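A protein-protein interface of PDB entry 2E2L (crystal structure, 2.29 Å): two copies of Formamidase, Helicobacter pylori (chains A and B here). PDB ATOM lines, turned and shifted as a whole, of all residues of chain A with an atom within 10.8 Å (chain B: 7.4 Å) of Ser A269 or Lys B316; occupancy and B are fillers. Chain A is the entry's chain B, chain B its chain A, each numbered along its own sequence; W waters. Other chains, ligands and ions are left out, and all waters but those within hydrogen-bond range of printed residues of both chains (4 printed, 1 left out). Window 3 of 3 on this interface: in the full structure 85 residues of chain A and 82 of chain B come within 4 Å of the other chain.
Water W3 bridges OH of Tyr A277 and O of Lys B318. Water W1 lies within hydrogen-bond range of O of Leu A268 (2.7 Å), N of Ile B317 (2.8 Å), O of Trp A270 (2.8 Å) and N of Lys B316 (3.3 Å). Water W4 bridges OH of Tyr A277 (2.8 Å) and OE1 of Glu B312 (3.0 Å). Water W2 lies within hydrogen-bond range of the backbone carbonyl oxygen of Ile B317 and the backbone carbonyl oxygen of Trp A270.
Of chain B, only Lys B316 and Ile B317 come within 4 Å of Ser A269. Printed residues of chain A within 4 Å of Asp B319: Tyr A284. Printed residues of chain B within 4 Å of Asn A274: Met B315. Of the printed residues of chain A, Lys B318 touches Tyr A277 (3.4 Å) and Tyr A284 (3.2 Å). Ala A266 touches none of the printed residues of chain B. Phe A238 touches none of the printed residues of chain B. The nearest residue of chain A that does not touch Lys B316 is Trp A270 (5.8 Å).
The backbone carbonyl oxygen of Leu A268 sits at hydrogen-bond distance from the backbone NH of Lys B316 (2.7 Å). The side-chain hydroxyl of Ser A269 sits at hydrogen-bond distance from the side-chain amino group of Lys B316 (3.1 Å).
The backbone carbonyl oxygen (O) of Trp A270 lies within hydrogen-bond range of the side-chain amide nitrogen (ND2) of Asn A274, at 3.0 Å. The guanidinium group (NE) of Arg A267 sits at hydrogen-bond distance from the backbone carbonyl oxygen (O) of Leu A212, at 3.2 Å. O of Glu B312 lies within hydrogen-bond range of NZ of Lys B318 (3.2 Å). The backbone carbonyl oxygen (O) of Asn A265 lies within hydrogen-bond range of the side-chain hydroxyl (OG) of Ser A269 (3.0 Å). O of Arg A267 sits at hydrogen-bond distance from ND2 of Asn A274 (3.0 Å). The side-chain hydroxyl (OG) of Ser B321 sits at hydrogen-bond distance from the side-chain carboxylate (OD1) of Asp B319 (2.7 Å).
NE1 of Trp B311 touches CB of Arg A267, at 3.5 Å. CE of Met B315 touches O of Arg A267, at 3.6 Å. Leu A268 touches Trp B311 (CD2 to O, 3.6 Å). Ile B317 touches Ser A269 (CD1 to O, 3.4 Å). Gly A271 touches Ile B317. Tyr A277 touches Glu B312 (CE1 to CD, 3.8 Å). Met B315 touches Tyr A277. Tyr A284 touches Ile B317. Tyr A284 touches Lys B318 (CD1 to O, 3.2 Å). Tyr A284 touches Asp B319 (CE1 to N, 3.5 Å).
Hydrophobic or aromatic side chains of chain A within 4 Å of the printed part of chain B: Leu A268, Tyr A277 and Tyr A284. Along chain A the printed residues that touch a printed residue of chain B span positions 267 to 284. Hydrophobic or aromatic side chains of chain B within 4 Å of the printed part of chain A: Trp B311, His B314, Met B315 and Ile B317.
No position is printed for both chains.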
ATOM      1  N   LEU A 212       6.014  20.306   0.521  1.00  0.00           N
ATOM      2  CA  LEU A 212       6.252  21.754   0.448  1.00  0.00           C
ATOM      3  C   LEU A 212       6.855  22.301   1.746  1.00  0.00           C
ATOM      4  O   LEU A 212       6.325  23.235   2.356  1.00  0.00           O
ATOM      5  CB  LEU A 212       4.974  22.516   0.052  1.00  0.00           C
ATOM      6  CG  LEU A 212       4.381  22.227  -1.331  1.00  0.00           C
ATOM      7  CD1 LEU A 212       3.019  22.904  -1.492  1.00  0.00           C
ATOM      8  CD2 LEU A 212       5.338  22.658  -2.442  1.00  0.00           C
ATOM      9  N   PHE A 238      11.764  24.114  -0.323  1.00  0.00           N
ATOM     10  CA  PHE A 238      10.440  23.486  -0.245  1.00  0.00           C
ATOM     11  C   PHE A 238       9.946  22.885  -1.568  1.00  0.00           C
ATOM     12  O   PHE A 238       8.933  22.187  -1.593  1.00  0.00           O
ATOM     13  CB  PHE A 238       9.398  24.456   0.346  1.00  0.00           C
ATOM     14  CG  PHE A 238       9.215  25.725  -0.446  1.00  0.00           C
ATOM     15  CD1 PHE A 238       8.362  25.763  -1.550  1.00  0.00           C
ATOM     16  CD2 PHE A 238       9.884  26.891  -0.078  1.00  0.00           C
ATOM     17  CE1 PHE A 238       8.191  26.936  -2.281  1.00  0.00           C
ATOM     18  CE2 PHE A 238       9.718  28.070  -0.802  1.00  0.00           C
ATOM     19  CZ  PHE A 238       8.870  28.092  -1.904  1.00  0.00           C
ATOM     20  N   LYS A 261       8.273  31.021   6.211  1.00  0.00           N
ATOM     21  CA  LYS A 261       7.044  31.709   5.793  1.00  0.00           C
ATOM     22  C   LYS A 261       6.719  31.463   4.318  1.00  0.00           C
ATOM     23  O   LYS A 261       5.550  31.410   3.935  1.00  0.00           O
ATOM     24  CB  LYS A 261       7.144  33.216   6.096  1.00  0.00           C
ATOM     25  CG  LYS A 261       6.096  34.119   5.424  1.00  0.00           C
ATOM     26  CD  LYS A 261       4.703  33.983   6.044  1.00  0.00           C
ATOM     27  CE  LYS A 261       3.707  34.925   5.373  1.00  0.00           C
ATOM     28  NZ  LYS A 261       2.373  34.932   6.052  1.00  0.00           N
ATOM     29  N   MET A 262       7.758  31.301   3.505  1.00  0.00           N
ATOM     30  CA  MET A 262       7.600  31.065   2.071  1.00  0.00           C
ATOM     31  C   MET A 262       7.090  29.661   1.764  1.00  0.00           C
ATOM     32  O   MET A 262       6.366  29.461   0.786  1.00  0.00           O
ATOM     33  CB  MET A 262       8.910  31.352   1.340  1.00  0.00           C
ATOM     34  CG  MET A 262       9.280  32.821   1.392  1.00  0.00           C
ATOM     35  SD  MET A 262      11.046  33.142   1.320  1.00  0.00           S
ATOM     36  CE  MET A 262      11.108  34.745   2.132  1.00  0.00           C
ATOM     37  N   ALA A 263       7.468  28.699   2.603  1.00  0.00           N
ATOM     38  CA  ALA A 263       6.925  27.345   2.533  1.00  0.00           C
ATOM     39  C   ALA A 263       5.434  27.360   2.873  1.00  0.00           C
ATOM     40  O   ALA A 263       4.632  26.697   2.209  1.00  0.00           O
ATOM     41  CB  ALA A 263       7.685  26.412   3.470  1.00  0.00           C
ATOM     42  N   ASP A 264       5.076  28.127   3.903  1.00  0.00           N
ATOM     43  CA  ASP A 264       3.681  28.346   4.278  1.00  0.00           C
ATOM     44  C   ASP A 264       2.912  29.019   3.146  1.00  0.00           C
ATOM     45  O   ASP A 264       1.803  28.598   2.810  1.00  0.00           O
ATOM     46  CB  ASP A 264       3.585  29.194   5.551  1.00  0.00           C
ATOM     47  CG  ASP A 264       4.334  28.583   6.724  1.00  0.00           C
ATOM     48  OD1 ASP A 264       4.394  27.338   6.824  1.00  0.00           O
ATOM     49  OD2 ASP A 264       4.860  29.357   7.553  1.00  0.00           O
ATOM     50  N   ASN A 265       3.514  30.059   2.565  1.00  0.00           N
ATOM     51  CA  ASN A 265       2.942  30.780   1.425  1.00  0.00           C
ATOM     52  C   ASN A 265       2.651  29.882   0.229  1.00  0.00           C
ATOM     53  O   ASN A 265       1.605  30.014  -0.406  1.00  0.00           O
ATOM     54  CB  ASN A 265       3.852  31.940   0.997  1.00  0.00           C
ATOM     55  CG  ASN A 265       3.555  33.230   1.747  1.00  0.00           C
ATOM     56  OD1 ASN A 265       2.450  33.432   2.257  1.00  0.00           O
ATOM     57  ND2 ASN A 265       4.544  34.119   1.806  1.00  0.00           N
ATOM     58  N   ALA A 266       3.581  28.976  -0.070  1.00  0.00           N
ATOM     59  CA  ALA A 266       3.411  28.001  -1.146  1.00  0.00           C
ATOM     60  C   ALA A 266       2.218  27.083  -0.879  1.00  0.00           C
ATOM     61  O   ALA A 266       1.394  26.853  -1.765  1.00  0.00           O
ATOM     62  CB  ALA A 266       4.682  27.190  -1.333  1.00  0.00           C
ATOM     63  N   ARG A 267       2.123  26.579   0.350  1.00  0.00           N
ATOM     64  CA  ARG A 267       1.010  25.720   0.769  1.00  0.00           C
ATOM     65  C   ARG A 267      -0.344  26.431   0.672  1.00  0.00           C
ATOM     66  O   ARG A 267      -1.363  25.802   0.385  1.00  0.00           O
ATOM     67  CB  ARG A 267       1.239  25.208   2.195  1.00  0.00           C
ATOM     68  CG  ARG A 267       2.356  24.181   2.318  1.00  0.00           C
ATOM     69  CD  ARG A 267       2.784  23.989   3.766  1.00  0.00           C
ATOM     70  NE  ARG A 267       3.604  22.790   3.934  1.00  0.00           N
ATOM     71  CZ  ARG A 267       4.080  22.349   5.096  1.00  0.00           C
ATOM     72  NH1 ARG A 267       3.827  22.998   6.226  1.00  0.00           N
ATOM     73  NH2 ARG A 267       4.814  21.243   5.128  1.00  0.00           N
ATOM     74  N   LEU A 268      -0.338  27.743   0.901  1.00  0.00           N
ATOM     75  CA  LEU A 268      -1.556  28.551   0.848  1.00  0.00           C
ATOM     76  C   LEU A 268      -1.930  29.005  -0.563  1.00  0.00           C
ATOM     77  O   LEU A 268      -3.109  29.026  -0.913  1.00  0.00           O
ATOM     78  CB  LEU A 268      -1.435  29.780   1.762  1.00  0.00           C
ATOM     79  CG  LEU A 268      -1.396  29.613   3.286  1.00  0.00           C
ATOM     80  CD1 LEU A 268      -1.187  30.965   3.952  1.00  0.00           C
ATOM     81  CD2 LEU A 268      -2.654  28.939   3.828  1.00  0.00           C
ATOM     82  N   SER A 269      -0.928  29.361  -1.365  1.00  0.00           N
ATOM     83  CA  SER A 269      -1.155  30.034  -2.649  1.00  0.00           C
ATOM     84  C   SER A 269      -1.146  29.123  -3.878  1.00  0.00           C
ATOM     85  O   SER A 269      -1.808  29.425  -4.873  1.00  0.00           O
ATOM     86  CB  SER A 269      -0.135  31.162  -2.849  1.00  0.00           C
ATOM     87  OG  SER A 269      -0.113  32.040  -1.734  1.00  0.00           O
ATOM     88  N   TRP A 270      -0.391  28.029  -3.813  1.00  0.00           N
ATOM     89  CA  TRP A 270      -0.202  27.147  -4.968  1.00  0.00           C
ATOM     90  C   TRP A 270      -1.464  26.381  -5.341  1.00  0.00           C
ATOM     91  O   TRP A 270      -2.291  26.066  -4.484  1.00  0.00           O
ATOM     92  CB  TRP A 270       0.946  26.162  -4.718  1.00  0.00           C
ATOM     93  CG  TRP A 270       2.322  26.756  -4.867  1.00  0.00           C
ATOM     94  CD1 TRP A 270       2.667  28.076  -4.763  1.00  0.00           C
ATOM     95  CD2 TRP A 270       3.540  26.045  -5.115  1.00  0.00           C
ATOM     96  NE1 TRP A 270       4.018  28.230  -4.950  1.00  0.00           N
ATOM     97  CE2 TRP A 270       4.580  26.999  -5.164  1.00  0.00           C
ATOM     98  CE3 TRP A 270       3.853  24.692  -5.305  1.00  0.00           C
ATOM     99  CZ2 TRP A 270       5.913  26.645  -5.396  1.00  0.00           C
ATOM    100  CZ3 TRP A 270       5.182  24.341  -5.540  1.00  0.00           C
ATOM    101  CH2 TRP A 270       6.194  25.315  -5.581  1.00  0.00           C
ATOM    102  N   GLY A 271      -1.599  26.090  -6.631  1.00  0.00           N
ATOM    103  CA  GLY A 271      -2.698  25.281  -7.133  1.00  0.00           C
ATOM    104  C   GLY A 271      -2.211  23.989  -7.755  1.00  0.00           C
ATOM    105  O   GLY A 271      -2.523  22.900  -7.268  1.00  0.00           O
ATOM    106  N   LEU A 272      -1.424  24.121  -8.821  1.00  0.00           N
ATOM    107  CA  LEU A 272      -0.987  22.982  -9.631  1.00  0.00           C
ATOM    108  C   LEU A 272      -0.099  21.964  -8.902  1.00  0.00           C
ATOM    109  O   LEU A 272      -0.256  20.755  -9.089  1.00  0.00           O
ATOM    110  CB  LEU A 272      -0.307  23.466 -10.919  1.00  0.00           C
ATOM    111  CG  LEU A 272      -1.195  24.165 -11.959  1.00  0.00           C
ATOM    112  CD1 LEU A 272      -0.349  24.762 -13.078  1.00  0.00           C
ATOM    113  CD2 LEU A 272      -2.247  23.221 -12.530  1.00  0.00           C
ATOM    114  N   GLU A 273       0.816  22.448  -8.071  1.00  0.00           N
ATOM    115  CA  GLU A 273       1.769  21.564  -7.393  1.00  0.00           C
ATOM    116  C   GLU A 273       1.457  21.367  -5.905  1.00  0.00           C
ATOM    117  O   GLU A 273       2.312  20.907  -5.141  1.00  0.00           O
ATOM    118  CB  GLU A 273       3.207  22.075  -7.562  1.00  0.00           C
ATOM    119  CG  GLU A 273       3.514  22.778  -8.884  1.00  0.00           C
ATOM    120  CD  GLU A 273       3.350  24.291  -8.804  1.00  0.00           C
ATOM    121  OE1 GLU A 273       2.251  24.766  -8.434  1.00  0.00           O
ATOM    122  OE2 GLU A 273       4.326  25.005  -9.124  1.00  0.00           O
ATOM    123  N   ASN A 274       0.237  21.710  -5.498  1.00  0.00           N
ATOM    124  CA  ASN A 274      -0.184  21.561  -4.107  1.00  0.00           C
ATOM    125  C   ASN A 274      -0.589  20.115  -3.816  1.00  0.00           C
ATOM    126  O   ASN A 274      -1.755  19.822  -3.538  1.00  0.00           O
ATOM    127  CB  ASN A 274      -1.323  22.531  -3.785  1.00  0.00           C
ATOM    128  CG  ASN A 274      -1.250  23.071  -2.371  1.00  0.00           C
ATOM    129  OD1 ASN A 274      -1.079  22.320  -1.409  1.00  0.00           O
ATOM    130  ND2 ASN A 274      -1.381  24.386  -2.236  1.00  0.00           N
ATOM    131  N   ASN A 275       0.393  19.221  -3.885  1.00  0.00           N
ATOM    132  CA  ASN A 275       0.165  17.777  -3.813  1.00  0.00           C
ATOM    133  C   ASN A 275      -0.348  17.312  -2.452  1.00  0.00           C
ATOM    134  O   ASN A 275      -1.175  16.401  -2.372  1.00  0.00           O
ATOM    135  CB  ASN A 275       1.441  17.017  -4.192  1.00  0.00           C
ATOM    136  CG  ASN A 275       2.055  17.514  -5.491  1.00  0.00           C
ATOM    137  OD1 ASN A 275       3.238  17.847  -5.543  1.00  0.00           O
ATOM    138  ND2 ASN A 275       1.252  17.574  -6.542  1.00  0.00           N
ATOM    139  N   ILE A 276       0.143  17.954  -1.395  1.00  0.00           N
ATOM    140  CA  ILE A 276      -0.263  17.650  -0.022  1.00  0.00           C
ATOM    141  C   ILE A 276      -1.768  17.890   0.216  1.00  0.00           C
ATOM    142  O   ILE A 276      -2.406  17.157   0.977  1.00  0.00           O
ATOM    143  CB  ILE A 276       0.635  18.397   1.018  1.00  0.00           C
ATOM    144  CG1 ILE A 276       0.410  17.844   2.432  1.00  0.00           C
ATOM    145  CG2 ILE A 276       0.454  19.923   0.927  1.00  0.00           C
ATOM    146  CD1 ILE A 276       1.470  18.240   3.445  1.00  0.00           C
ATOM    147  N   TYR A 277      -2.328  18.899  -0.449  1.00  0.00           N
ATOM    148  CA  TYR A 277      -3.772  19.135  -0.411  1.00  0.00           C
ATOM    149  C   TYR A 277      -4.510  18.111  -1.272  1.00  0.00           C
ATOM    150  O   TYR A 277      -5.487  17.507  -0.824  1.00  0.00           O
ATOM    151  CB  TYR A 277      -4.111  20.562  -0.855  1.00  0.00           C
ATOM    152  CG  TYR A 277      -5.596  20.876  -0.849  1.00  0.00           C
ATOM    153  CD1 TYR A 277      -6.260  21.185   0.340  1.00  0.00           C
ATOM    154  CD2 TYR A 277      -6.335  20.865  -2.034  1.00  0.00           C
ATOM    155  CE1 TYR A 277      -7.622  21.476   0.348  1.00  0.00           C
ATOM    156  CE2 TYR A 277      -7.696  21.152  -2.034  1.00  0.00           C
ATOM    157  CZ  TYR A 277      -8.333  21.455  -0.842  1.00  0.00           C
ATOM    158  OH  TYR A 277      -9.677  21.742  -0.841  1.00  0.00           O
ATOM    159  N   TYR A 284     -10.967  18.009  -7.270  1.00  0.00           N
ATOM    160  CA  TYR A 284     -11.928  18.937  -6.668  1.00  0.00           C
ATOM    161  C   TYR A 284     -12.653  19.837  -7.676  1.00  0.00           C
ATOM    162  O   TYR A 284     -13.675  20.438  -7.342  1.00  0.00           O
ATOM    163  CB  TYR A 284     -11.304  19.759  -5.528  1.00  0.00           C
ATOM    164  CG  TYR A 284     -10.081  20.579  -5.888  1.00  0.00           C
ATOM    165  CD1 TYR A 284     -10.173  21.682  -6.740  1.00  0.00           C
ATOM    166  CD2 TYR A 284      -8.832  20.271  -5.346  1.00  0.00           C
ATOM    167  CE1 TYR A 284      -9.051  22.440  -7.059  1.00  0.00           C
ATOM    168  CE2 TYR A 284      -7.705  21.025  -5.658  1.00  0.00           C
ATOM    169  CZ  TYR A 284      -7.823  22.109  -6.513  1.00  0.00           C
ATOM    170  OH  TYR A 284      -6.711  22.858  -6.828  1.00  0.00           O
ATOM    171  N   TRP B 311      -3.906  24.311   7.670  1.00  0.00           N
ATOM    172  CA  TRP B 311      -3.975  25.596   6.966  1.00  0.00           C
ATOM    173  C   TRP B 311      -5.023  25.634   5.848  1.00  0.00           C
ATOM    174  O   TRP B 311      -5.107  26.618   5.107  1.00  0.00           O
ATOM    175  CB  TRP B 311      -2.598  25.957   6.393  1.00  0.00           C
ATOM    176  CG  TRP B 311      -2.064  24.927   5.441  1.00  0.00           C
ATOM    177  CD1 TRP B 311      -2.344  24.818   4.108  1.00  0.00           C
ATOM    178  CD2 TRP B 311      -1.163  23.856   5.749  1.00  0.00           C
ATOM    179  NE1 TRP B 311      -1.674  23.748   3.567  1.00  0.00           N
ATOM    180  CE2 TRP B 311      -0.940  23.140   4.552  1.00  0.00           C
ATOM    181  CE3 TRP B 311      -0.519  23.435   6.920  1.00  0.00           C
ATOM    182  CZ2 TRP B 311      -0.103  22.023   4.491  1.00  0.00           C
ATOM    183  CZ3 TRP B 311       0.316  22.324   6.859  1.00  0.00           C
ATOM    184  CH2 TRP B 311       0.516  21.632   5.652  1.00  0.00           C
ATOM    185  N   GLU B 312      -5.816  24.569   5.735  1.00  0.00           N
ATOM    186  CA  GLU B 312      -6.788  24.416   4.643  1.00  0.00           C
ATOM    187  C   GLU B 312      -7.776  25.570   4.470  1.00  0.00           C
ATOM    188  O   GLU B 312      -8.157  25.893   3.343  1.00  0.00           O
ATOM    189  CB  GLU B 312      -7.560  23.104   4.783  1.00  0.00           C
ATOM    190  CG  GLU B 312      -6.904  21.937   4.078  1.00  0.00           C
ATOM    191  CD  GLU B 312      -7.781  20.704   4.027  1.00  0.00           C
ATOM    192  OE1 GLU B 312      -9.014  20.837   3.859  1.00  0.00           O
ATOM    193  OE2 GLU B 312      -7.229  19.591   4.141  1.00  0.00           O
ATOM    194  N   ASP B 313      -8.189  26.179   5.579  1.00  0.00           N
ATOM    195  CA  ASP B 313      -9.190  27.250   5.549  1.00  0.00           C
ATOM    196  C   ASP B 313      -8.688  28.545   4.909  1.00  0.00           C
ATOM    197  O   ASP B 313      -9.488  29.363   4.447  1.00  0.00           O
ATOM    198  CB  ASP B 313      -9.735  27.521   6.958  1.00  0.00           C
ATOM    199  CG  ASP B 313     -10.668  26.421   7.453  1.00  0.00           C
ATOM    200  OD1 ASP B 313     -11.293  25.726   6.620  1.00  0.00           O
ATOM    201  OD2 ASP B 313     -10.785  26.258   8.686  1.00  0.00           O
ATOM    202  N   HIS B 314      -7.370  28.719   4.869  1.00  0.00           N
ATOM    203  CA  HIS B 314      -6.767  29.946   4.348  1.00  0.00           C
ATOM    204  C   HIS B 314      -6.114  29.765   2.975  1.00  0.00           C
ATOM    205  O   HIS B 314      -5.410  30.659   2.487  1.00  0.00           O
ATOM    206  CB  HIS B 314      -5.771  30.513   5.363  1.00  0.00           C
ATOM    207  CG  HIS B 314      -6.403  30.918   6.659  1.00  0.00           C
ATOM    208  ND1 HIS B 314      -7.090  32.103   6.813  1.00  0.00           N
ATOM    209  CD2 HIS B 314      -6.463  30.289   7.857  1.00  0.00           C
ATOM    210  CE1 HIS B 314      -7.540  32.190   8.052  1.00  0.00           C
ATOM    211  NE2 HIS B 314      -7.172  31.102   8.707  1.00  0.00           N
ATOM    212  N   MET B 315      -6.364  28.613   2.357  1.00  0.00           N
ATOM    213  CA  MET B 315      -5.834  28.304   1.030  1.00  0.00           C
ATOM    214  C   MET B 315      -6.560  29.078  -0.073  1.00  0.00           C
ATOM    215  O   MET B 315      -7.788  29.204  -0.052  1.00  0.00           O
ATOM    216  CB  MET B 315      -5.905  26.800   0.759  1.00  0.00           C
ATOM    217  CG  MET B 315      -4.843  25.983   1.490  1.00  0.00           C
ATOM    218  SD  MET B 315      -4.827  24.245   0.999  1.00  0.00           S
ATOM    219  CE  MET B 315      -4.461  24.383  -0.751  1.00  0.00           C
ATOM    220  N   LYS B 316      -5.785  29.579  -1.035  1.00  0.00           N
ATOM    221  CA  LYS B 316      -6.300  30.420  -2.116  1.00  0.00           C
ATOM    222  C   LYS B 316      -7.041  29.635  -3.196  1.00  0.00           C
ATOM    223  O   LYS B 316      -8.121  30.044  -3.632  1.00  0.00           O
ATOM    224  CB  LYS B 316      -5.169  31.227  -2.760  1.00  0.00           C
ATOM    225  CG  LYS B 316      -4.596  32.337  -1.892  1.00  0.00           C
ATOM    226  CD  LYS B 316      -3.472  33.055  -2.625  1.00  0.00           C
ATOM    227  CE  LYS B 316      -2.796  34.100  -1.751  1.00  0.00           C
ATOM    228  NZ  LYS B 316      -1.576  34.646  -2.412  1.00  0.00           N
ATOM    229  N   ILE B 317      -6.458  28.518  -3.628  1.00  0.00           N
ATOM    230  CA  ILE B 317      -7.006  27.735  -4.739  1.00  0.00           C
ATOM    231  C   ILE B 317      -7.595  26.399  -4.275  1.00  0.00           C
ATOM    232  O   ILE B 317      -6.865  25.478  -3.895  1.00  0.00           O
ATOM    233  CB  ILE B 317      -5.957  27.506  -5.864  1.00  0.00           C
ATOM    234  CG1 ILE B 317      -5.374  28.843  -6.340  1.00  0.00           C
ATOM    235  CG2 ILE B 317      -6.583  26.733  -7.030  1.00  0.00           C
ATOM    236  CD1 ILE B 317      -4.129  28.719  -7.211  1.00  0.00           C
ATOM    237  N   LYS B 318      -8.923  26.314  -4.312  1.00  0.00           N
ATOM    238  CA  LYS B 318      -9.651  25.098  -3.943  1.00  0.00           C
ATOM    239  C   LYS B 318     -10.703  24.729  -4.993  1.00  0.00           C
ATOM    240  O   LYS B 318     -11.516  23.828  -4.781  1.00  0.00           O
ATOM    241  CB  LYS B 318     -10.292  25.245  -2.556  1.00  0.00           C
ATOM    242  CG  LYS B 318      -9.306  25.111  -1.396  1.00  0.00           C
ATOM    243  CD  LYS B 318      -9.990  25.215  -0.034  1.00  0.00           C
ATOM    244  CE  LYS B 318     -10.183  26.664   0.400  1.00  0.00           C
ATOM    245  NZ  LYS B 318     -10.832  26.763   1.741  1.00  0.00           N
ATOM    246  N   ASP B 319     -10.672  25.434  -6.123  1.00  0.00           N
ATOM    247  CA  ASP B 319     -11.560  25.164  -7.255  1.00  0.00           C
ATOM    248  C   ASP B 319     -10.876  25.526  -8.575  1.00  0.00           C
ATOM    249  O   ASP B 319      -9.748  26.022  -8.577  1.00  0.00           O
ATOM    250  CB  ASP B 319     -12.888  25.917  -7.100  1.00  0.00           C
ATOM    251  CG  ASP B 319     -12.702  27.419  -6.938  1.00  0.00           C
ATOM    252  OD1 ASP B 319     -12.104  28.061  -7.827  1.00  0.00           O
ATOM    253  OD2 ASP B 319     -13.171  27.963  -5.918  1.00  0.00           O
ATOM    254  N   SER B 321     -11.831  27.825 -10.866  1.00  0.00           N
ATOM    255  CA  SER B 321     -12.347  29.098 -11.380  1.00  0.00           C
ATOM    256  C   SER B 321     -11.294  29.941 -12.102  1.00  0.00           C
ATOM    257  O   SER B 321     -11.628  30.695 -13.018  1.00  0.00           O
ATOM    258  CB  SER B 321     -13.005  29.917 -10.264  1.00  0.00           C
ATOM    259  OG  SER B 321     -12.059  30.303  -9.283  1.00  0.00           O
HETATM  260  O   HOH W   1      -4.141  27.223  -2.681  1.00  0.00           O
HETATM  261  O   HOH W   2      -4.511  23.814  -4.105  1.00  0.00           O
HETATM  262  O   HOH W   3     -11.442  21.659  -2.817  1.00  0.00           O
HETATM  263  O   HOH W   4     -10.598  22.225   1.724  1.00  0.00           O
